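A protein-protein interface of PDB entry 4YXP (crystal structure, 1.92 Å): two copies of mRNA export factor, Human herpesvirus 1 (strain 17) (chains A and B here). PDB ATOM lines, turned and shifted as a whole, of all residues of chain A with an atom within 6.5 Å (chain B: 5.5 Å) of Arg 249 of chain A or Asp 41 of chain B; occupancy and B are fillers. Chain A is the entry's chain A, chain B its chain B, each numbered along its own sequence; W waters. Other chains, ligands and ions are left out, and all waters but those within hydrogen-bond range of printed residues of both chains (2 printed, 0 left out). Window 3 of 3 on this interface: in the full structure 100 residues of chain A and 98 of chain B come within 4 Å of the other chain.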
ATOM      1  N   CYS A 246     -11.625 -26.907  38.209  1.00  0.00           N
ATOM      2  CA  CYS A 246     -11.723 -25.448  38.209  1.00  0.00           C
ATOM      3  C   CYS A 246     -12.693 -24.953  37.133  1.00  0.00           C
ATOM      4  O   CYS A 246     -12.606 -25.352  35.972  1.00  0.00           O
ATOM      5  CB  CYS A 246     -10.333 -24.833  37.996  1.00  0.00           C
ATOM      6  SG  CYS A 246     -10.267 -23.015  37.968  1.00  0.00           S
ATOM      7  N   SER A 247     -13.609 -24.074  37.528  1.00  0.00           N
ATOM      8  CA  SER A 247     -14.639 -23.572  36.619  1.00  0.00           C
ATOM      9  C   SER A 247     -14.284 -22.224  35.986  1.00  0.00           C
ATOM     10  O   SER A 247     -15.092 -21.647  35.262  1.00  0.00           O
ATOM     11  CB  SER A 247     -15.969 -23.445  37.361  1.00  0.00           C
ATOM     12  OG  SER A 247     -15.869 -22.496  38.407  1.00  0.00           O
ATOM     13  N   SER A 248     -13.080 -21.723  36.251  1.00  0.00           N
ATOM     14  CA  SER A 248     -12.655 -20.434  35.708  1.00  0.00           C
ATOM     15  C   SER A 248     -12.144 -20.558  34.271  1.00  0.00           C
ATOM     16  O   SER A 248     -11.150 -21.238  34.013  1.00  0.00           O
ATOM     17  CB  SER A 248     -11.563 -19.818  36.589  1.00  0.00           C
ATOM     18  OG  SER A 248     -10.986 -18.682  35.966  1.00  0.00           O
ATOM     19  N   ARG A 249     -12.823 -19.891  33.342  1.00  0.00           N
ATOM     20  CA  ARG A 249     -12.406 -19.882  31.939  1.00  0.00           C
ATOM     21  C   ARG A 249     -11.072 -19.151  31.772  1.00  0.00           C
ATOM     22  O   ARG A 249     -10.222 -19.558  30.979  1.00  0.00           O
ATOM     23  CB  ARG A 249     -13.487 -19.233  31.068  1.00  0.00           C
ATOM     24  CG  ARG A 249     -13.074 -18.962  29.620  1.00  0.00           C
ATOM     25  CD  ARG A 249     -12.793 -20.236  28.839  1.00  0.00           C
ATOM     26  NE  ARG A 249     -12.552 -19.949  27.425  1.00  0.00           N
ATOM     27  CZ  ARG A 249     -12.326 -20.869  26.492  1.00  0.00           C
ATOM     28  NH1 ARG A 249     -12.308 -22.158  26.806  1.00  0.00           N
ATOM     29  NH2 ARG A 249     -12.118 -20.498  25.238  1.00  0.00           N
ATOM     30  N   VAL A 250     -10.897 -18.064  32.514  1.00  0.00           N
ATOM     31  CA  VAL A 250      -9.633 -17.339  32.513  1.00  0.00           C
ATOM     32  C   VAL A 250      -8.499 -18.283  32.898  1.00  0.00           C
ATOM     33  O   VAL A 250      -7.432 -18.266  32.286  1.00  0.00           O
ATOM     34  CB  VAL A 250      -9.691 -16.123  33.461  1.00  0.00           C
ATOM     35  CG1 VAL A 250      -8.291 -15.572  33.743  1.00  0.00           C
ATOM     36  CG2 VAL A 250     -10.573 -15.032  32.856  1.00  0.00           C
ATOM     37  N   CYS A 251      -8.732 -19.107  33.914  1.00  0.00           N
ATOM     38  CA  CYS A 251      -7.714 -20.042  34.378  1.00  0.00           C
ATOM     39  C   CYS A 251      -7.412 -21.096  33.310  1.00  0.00           C
ATOM     40  O   CYS A 251      -6.252 -21.432  33.078  1.00  0.00           O
ATOM     41  CB  CYS A 251      -8.154 -20.713  35.683  1.00  0.00           C
ATOM     42  SG  CYS A 251      -6.900 -21.807  36.425  1.00  0.00           S
ATOM     43  N   GLU A 252      -8.449 -21.612  32.654  1.00  0.00           N
ATOM     44  CA  GLU A 252      -8.259 -22.617  31.611  1.00  0.00           C
ATOM     45  C   GLU A 252      -7.492 -22.029  30.424  1.00  0.00           C
ATOM     46  O   GLU A 252      -6.669 -22.706  29.816  1.00  0.00           O
ATOM     47  CB  GLU A 252      -9.603 -23.186  31.140  1.00  0.00           C
ATOM     48  CG  GLU A 252      -9.461 -24.417  30.243  1.00  0.00           C
ATOM     49  CD  GLU A 252     -10.799 -24.979  29.782  1.00  0.00           C
ATOM     50  OE1 GLU A 252     -11.830 -24.294  29.947  1.00  0.00           O
ATOM     51  OE2 GLU A 252     -10.816 -26.111  29.251  1.00  0.00           O
ATOM     52  N   LEU A 253      -7.769 -20.772  30.090  1.00  0.00           N
ATOM     53  CA  LEU A 253      -7.019 -20.087  29.037  1.00  0.00           C
ATOM     54  C   LEU A 253      -5.549 -19.935  29.418  1.00  0.00           C
ATOM     55  O   LEU A 253      -4.663 -20.181  28.605  1.00  0.00           O
ATOM     56  CB  LEU A 253      -7.613 -18.710  28.753  1.00  0.00           C
ATOM     57  CG  LEU A 253      -8.902 -18.676  27.932  1.00  0.00           C
ATOM     58  CD1 LEU A 253      -9.492 -17.280  27.957  1.00  0.00           C
ATOM     59  CD2 LEU A 253      -8.641 -19.118  26.498  1.00  0.00           C
ATOM     60  N   THR A 254      -5.307 -19.519  30.658  1.00  0.00           N
ATOM     61  CA  THR A 254      -3.953 -19.296  31.154  1.00  0.00           C
ATOM     62  C   THR A 254      -3.135 -20.586  31.115  1.00  0.00           C
ATOM     63  O   THR A 254      -2.013 -20.606  30.602  1.00  0.00           O
ATOM     64  CB  THR A 254      -3.979 -18.746  32.596  1.00  0.00           C
ATOM     65  OG1 THR A 254      -4.678 -17.495  32.612  1.00  0.00           O
ATOM     66  CG2 THR A 254      -2.561 -18.541  33.142  1.00  0.00           C
ATOM     67  N   GLN B  37      -6.275 -27.179  21.630  1.00  0.00           N
ATOM     68  CA  GLN B  37      -7.669 -27.072  21.217  1.00  0.00           C
ATOM     69  C   GLN B  37      -8.337 -25.837  21.824  1.00  0.00           C
ATOM     70  O   GLN B  37      -9.143 -25.179  21.172  1.00  0.00           O
ATOM     71  CB  GLN B  37      -8.442 -28.333  21.611  1.00  0.00           C
ATOM     72  CG  GLN B  37      -9.838 -28.416  21.009  1.00  0.00           C
ATOM     73  CD  GLN B  37      -9.812 -28.562  19.499  1.00  0.00           C
ATOM     74  OE1 GLN B  37      -9.088 -29.399  18.956  1.00  0.00           O
ATOM     75  NE2 GLN B  37     -10.601 -27.743  18.810  1.00  0.00           N
ATOM     76  N   VAL B  38      -8.007 -25.528  23.072  1.00  0.00           N
ATOM     77  CA  VAL B  38      -8.534 -24.331  23.721  1.00  0.00           C
ATOM     78  C   VAL B  38      -8.084 -23.094  22.949  1.00  0.00           C
ATOM     79  O   VAL B  38      -8.854 -22.149  22.758  1.00  0.00           O
ATOM     80  CB  VAL B  38      -8.089 -24.255  25.199  1.00  0.00           C
ATOM     81  CG1 VAL B  38      -8.408 -22.884  25.799  1.00  0.00           C
ATOM     82  CG2 VAL B  38      -8.763 -25.350  26.008  1.00  0.00           C
ATOM     83  N   MET B  39      -6.835 -23.113  22.495  1.00  0.00           N
ATOM     84  CA  MET B  39      -6.244 -21.956  21.835  1.00  0.00           C
ATOM     85  C   MET B  39      -6.685 -21.803  20.379  1.00  0.00           C
ATOM     86  O   MET B  39      -6.313 -20.832  19.715  1.00  0.00           O
ATOM     87  CB  MET B  39      -4.718 -22.047  21.909  1.00  0.00           C
ATOM     88  CG  MET B  39      -4.172 -22.007  23.330  1.00  0.00           C
ATOM     89  SD  MET B  39      -4.723 -20.564  24.275  1.00  0.00           S
ATOM     90  CE  MET B  39      -4.160 -19.232  23.218  1.00  0.00           C
ATOM     91  N   HIS B  40      -7.484 -22.745  19.886  1.00  0.00           N
ATOM     92  CA  HIS B  40      -7.964 -22.686  18.510  1.00  0.00           C
ATOM     93  C   HIS B  40      -9.010 -21.584  18.335  1.00  0.00           C
ATOM     94  O   HIS B  40      -9.104 -20.966  17.275  1.00  0.00           O
ATOM     95  CB  HIS B  40      -8.552 -24.034  18.090  1.00  0.00           C
ATOM     96  CG  HIS B  40      -9.226 -24.009  16.753  1.00  0.00           C
ATOM     97  ND1 HIS B  40      -8.536 -23.808  15.574  1.00  0.00           N
ATOM     98  CD2 HIS B  40     -10.526 -24.154  16.407  1.00  0.00           C
ATOM     99  CE1 HIS B  40      -9.383 -23.834  14.563  1.00  0.00           C
ATOM    100  NE2 HIS B  40     -10.598 -24.042  15.039  1.00  0.00           N
ATOM    101  N   ASP B  41      -9.788 -21.345  19.386  1.00  0.00           N
ATOM    102  CA  ASP B  41     -10.858 -20.354  19.352  1.00  0.00           C
ATOM    103  C   ASP B  41     -11.078 -19.799  20.754  1.00  0.00           C
ATOM    104  O   ASP B  41     -12.132 -20.004  21.350  1.00  0.00           O
ATOM    105  CB  ASP B  41     -12.144 -20.978  18.809  1.00  0.00           C
ATOM    106  CG  ASP B  41     -13.251 -19.957  18.602  1.00  0.00           C
ATOM    107  OD1 ASP B  41     -12.961 -18.741  18.607  1.00  0.00           O
ATOM    108  OD2 ASP B  41     -14.412 -20.378  18.421  1.00  0.00           O
ATOM    109  N   PRO B  42     -10.075 -19.088  21.286  1.00  0.00           N
ATOM    110  CA  PRO B  42     -10.077 -18.660  22.689  1.00  0.00           C
ATOM    111  C   PRO B  42     -11.220 -17.714  23.046  1.00  0.00           C
ATOM    112  O   PRO B  42     -11.669 -17.717  24.189  1.00  0.00           O
ATOM    113  CB  PRO B  42      -8.723 -17.960  22.846  1.00  0.00           C
ATOM    114  CG  PRO B  42      -8.332 -17.557  21.474  1.00  0.00           C
ATOM    115  CD  PRO B  42      -8.893 -18.595  20.558  1.00  0.00           C
ATOM    116  N   PHE B  43     -11.684 -16.918  22.091  1.00  0.00           N
ATOM    117  CA  PHE B  43     -12.793 -16.009  22.359  1.00  0.00           C
ATOM    118  C   PHE B  43     -14.115 -16.764  22.342  1.00  0.00           C
ATOM    119  O   PHE B  43     -15.146 -16.233  22.750  1.00  0.00           O
ATOM    120  CB  PHE B  43     -12.807 -14.861  21.348  1.00  0.00           C
ATOM    121  CG  PHE B  43     -11.738 -13.837  21.593  1.00  0.00           C
ATOM    122  CD1 PHE B  43     -11.933 -12.823  22.517  1.00  0.00           C
ATOM    123  CD2 PHE B  43     -10.537 -13.891  20.912  1.00  0.00           C
ATOM    124  CE1 PHE B  43     -10.953 -11.881  22.754  1.00  0.00           C
ATOM    125  CE2 PHE B  43      -9.548 -12.946  21.143  1.00  0.00           C
ATOM    126  CZ  PHE B  43      -9.757 -11.944  22.066  1.00  0.00           C
ATOM    127  N   GLY B  44     -14.069 -18.006  21.867  1.00  0.00           N
ATOM    128  CA  GLY B  44     -15.193 -18.921  21.943  1.00  0.00           C
ATOM    129  C   GLY B  44     -16.568 -18.318  21.747  1.00  0.00           C
ATOM    130  O   GLY B  44     -17.431 -18.439  22.617  1.00  0.00           O
ATOM    131  N   GLY B  45     -16.774 -17.664  20.610  1.00  0.00           N
ATOM    132  CA  GLY B  45     -18.088 -17.163  20.253  1.00  0.00           C
ATOM    133  C   GLY B  45     -18.354 -15.710  20.600  1.00  0.00           C
ATOM    134  O   GLY B  45     -19.347 -15.140  20.147  1.00  0.00           O
HETATM  135  O   HOH W   1     -13.165 -17.164  26.388  1.00  0.00           O
HETATM  136  O   HOH W   2     -11.414 -22.325  23.516  1.00  0.00           O
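O of Pro 42 of chain B lies within hydrogen-bond range of NH2 of Arg 249 of chain A.
OE1 of Glu 252 of chain A is in salt-bridge range of NH1 of Arg 249 of chain A (3.8 Å).
Arg 249 of chain A touches Asp 41 of chain B.
CG2 of Val 38 of chain B touches OE2 of Glu 252 of chain A (3.9 Å).
CD2 of Leu 253 of chain A touches CG1 of Val 38 of chain B (3.8 Å).
CD2 of Leu 253 of chain A touches CB of Pro 42 of chain B, at 3.8 Å.
Ser 248 of chain A touches none of the printed residues of chain B.
Arg 249 of chain A touches just these residues of chain B: Asp 41 (3.9 Å) and Pro 42 (3.0 Å).
Of the printed residues of chain B, Glu 252 of chain A touches Val 38.
Of the printed residues of chain B, Leu 253 of chain A touches Val 38 and Pro 42.
Of the printed residues of chain A, Val 38 of chain B touches Glu 252 (3.9 Å) and Leu 253 (3.8 Å).
His 40 of chain B touches none of the printed residues of chain A.
Printed residues of chain A within 4 Å of Asp 41 of chain B: Arg 249 (3.9 Å).
Of the printed residues of chain A, Pro 42 of chain B touches Arg 249 and Leu 253.
Of the 9 printed residues of chain B, 3 touch a printed residue of chain A.
Printed residues of chain B that touch a printed residue of chain A: Val 38, Asp 41 and Pro 42.
Hydrophobic or aromatic side chains of chain B that line the printed part of chain A: Val 38 and Pro 42.
Of the 9 printed residues of chain A, 3 touch a printed residue of chain B.
Hydrophobic or aromatic side chains of chain A within 4 Å of the printed part of chain B: Leu 253.
Among the printed residues, no Asp or Glu carboxylate lies within 4 Å of a Lys or Arg side-chain nitrogen of the other chain.
No position is printed for both chains.
Of the 5 pairs that touch across the chains among the printed residues, none has its exchanged pair printed and touching as well.
Water W2 lies within hydrogen-bond range of the guanidinium group (NH2) of Arg 249 of chain A (2.6 Å), the backbone carbonyl oxygen (O) of Val 38 of chain B (2.7 Å) and the backbone carbonyl oxygen (O) of Asp 41 of chain B (3.3 Å).
Water W1 lies within hydrogen-bond range of O of Pro 42 of chain B (2.7 Å) and NE of Arg 249 of chain A (3.0 Å).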
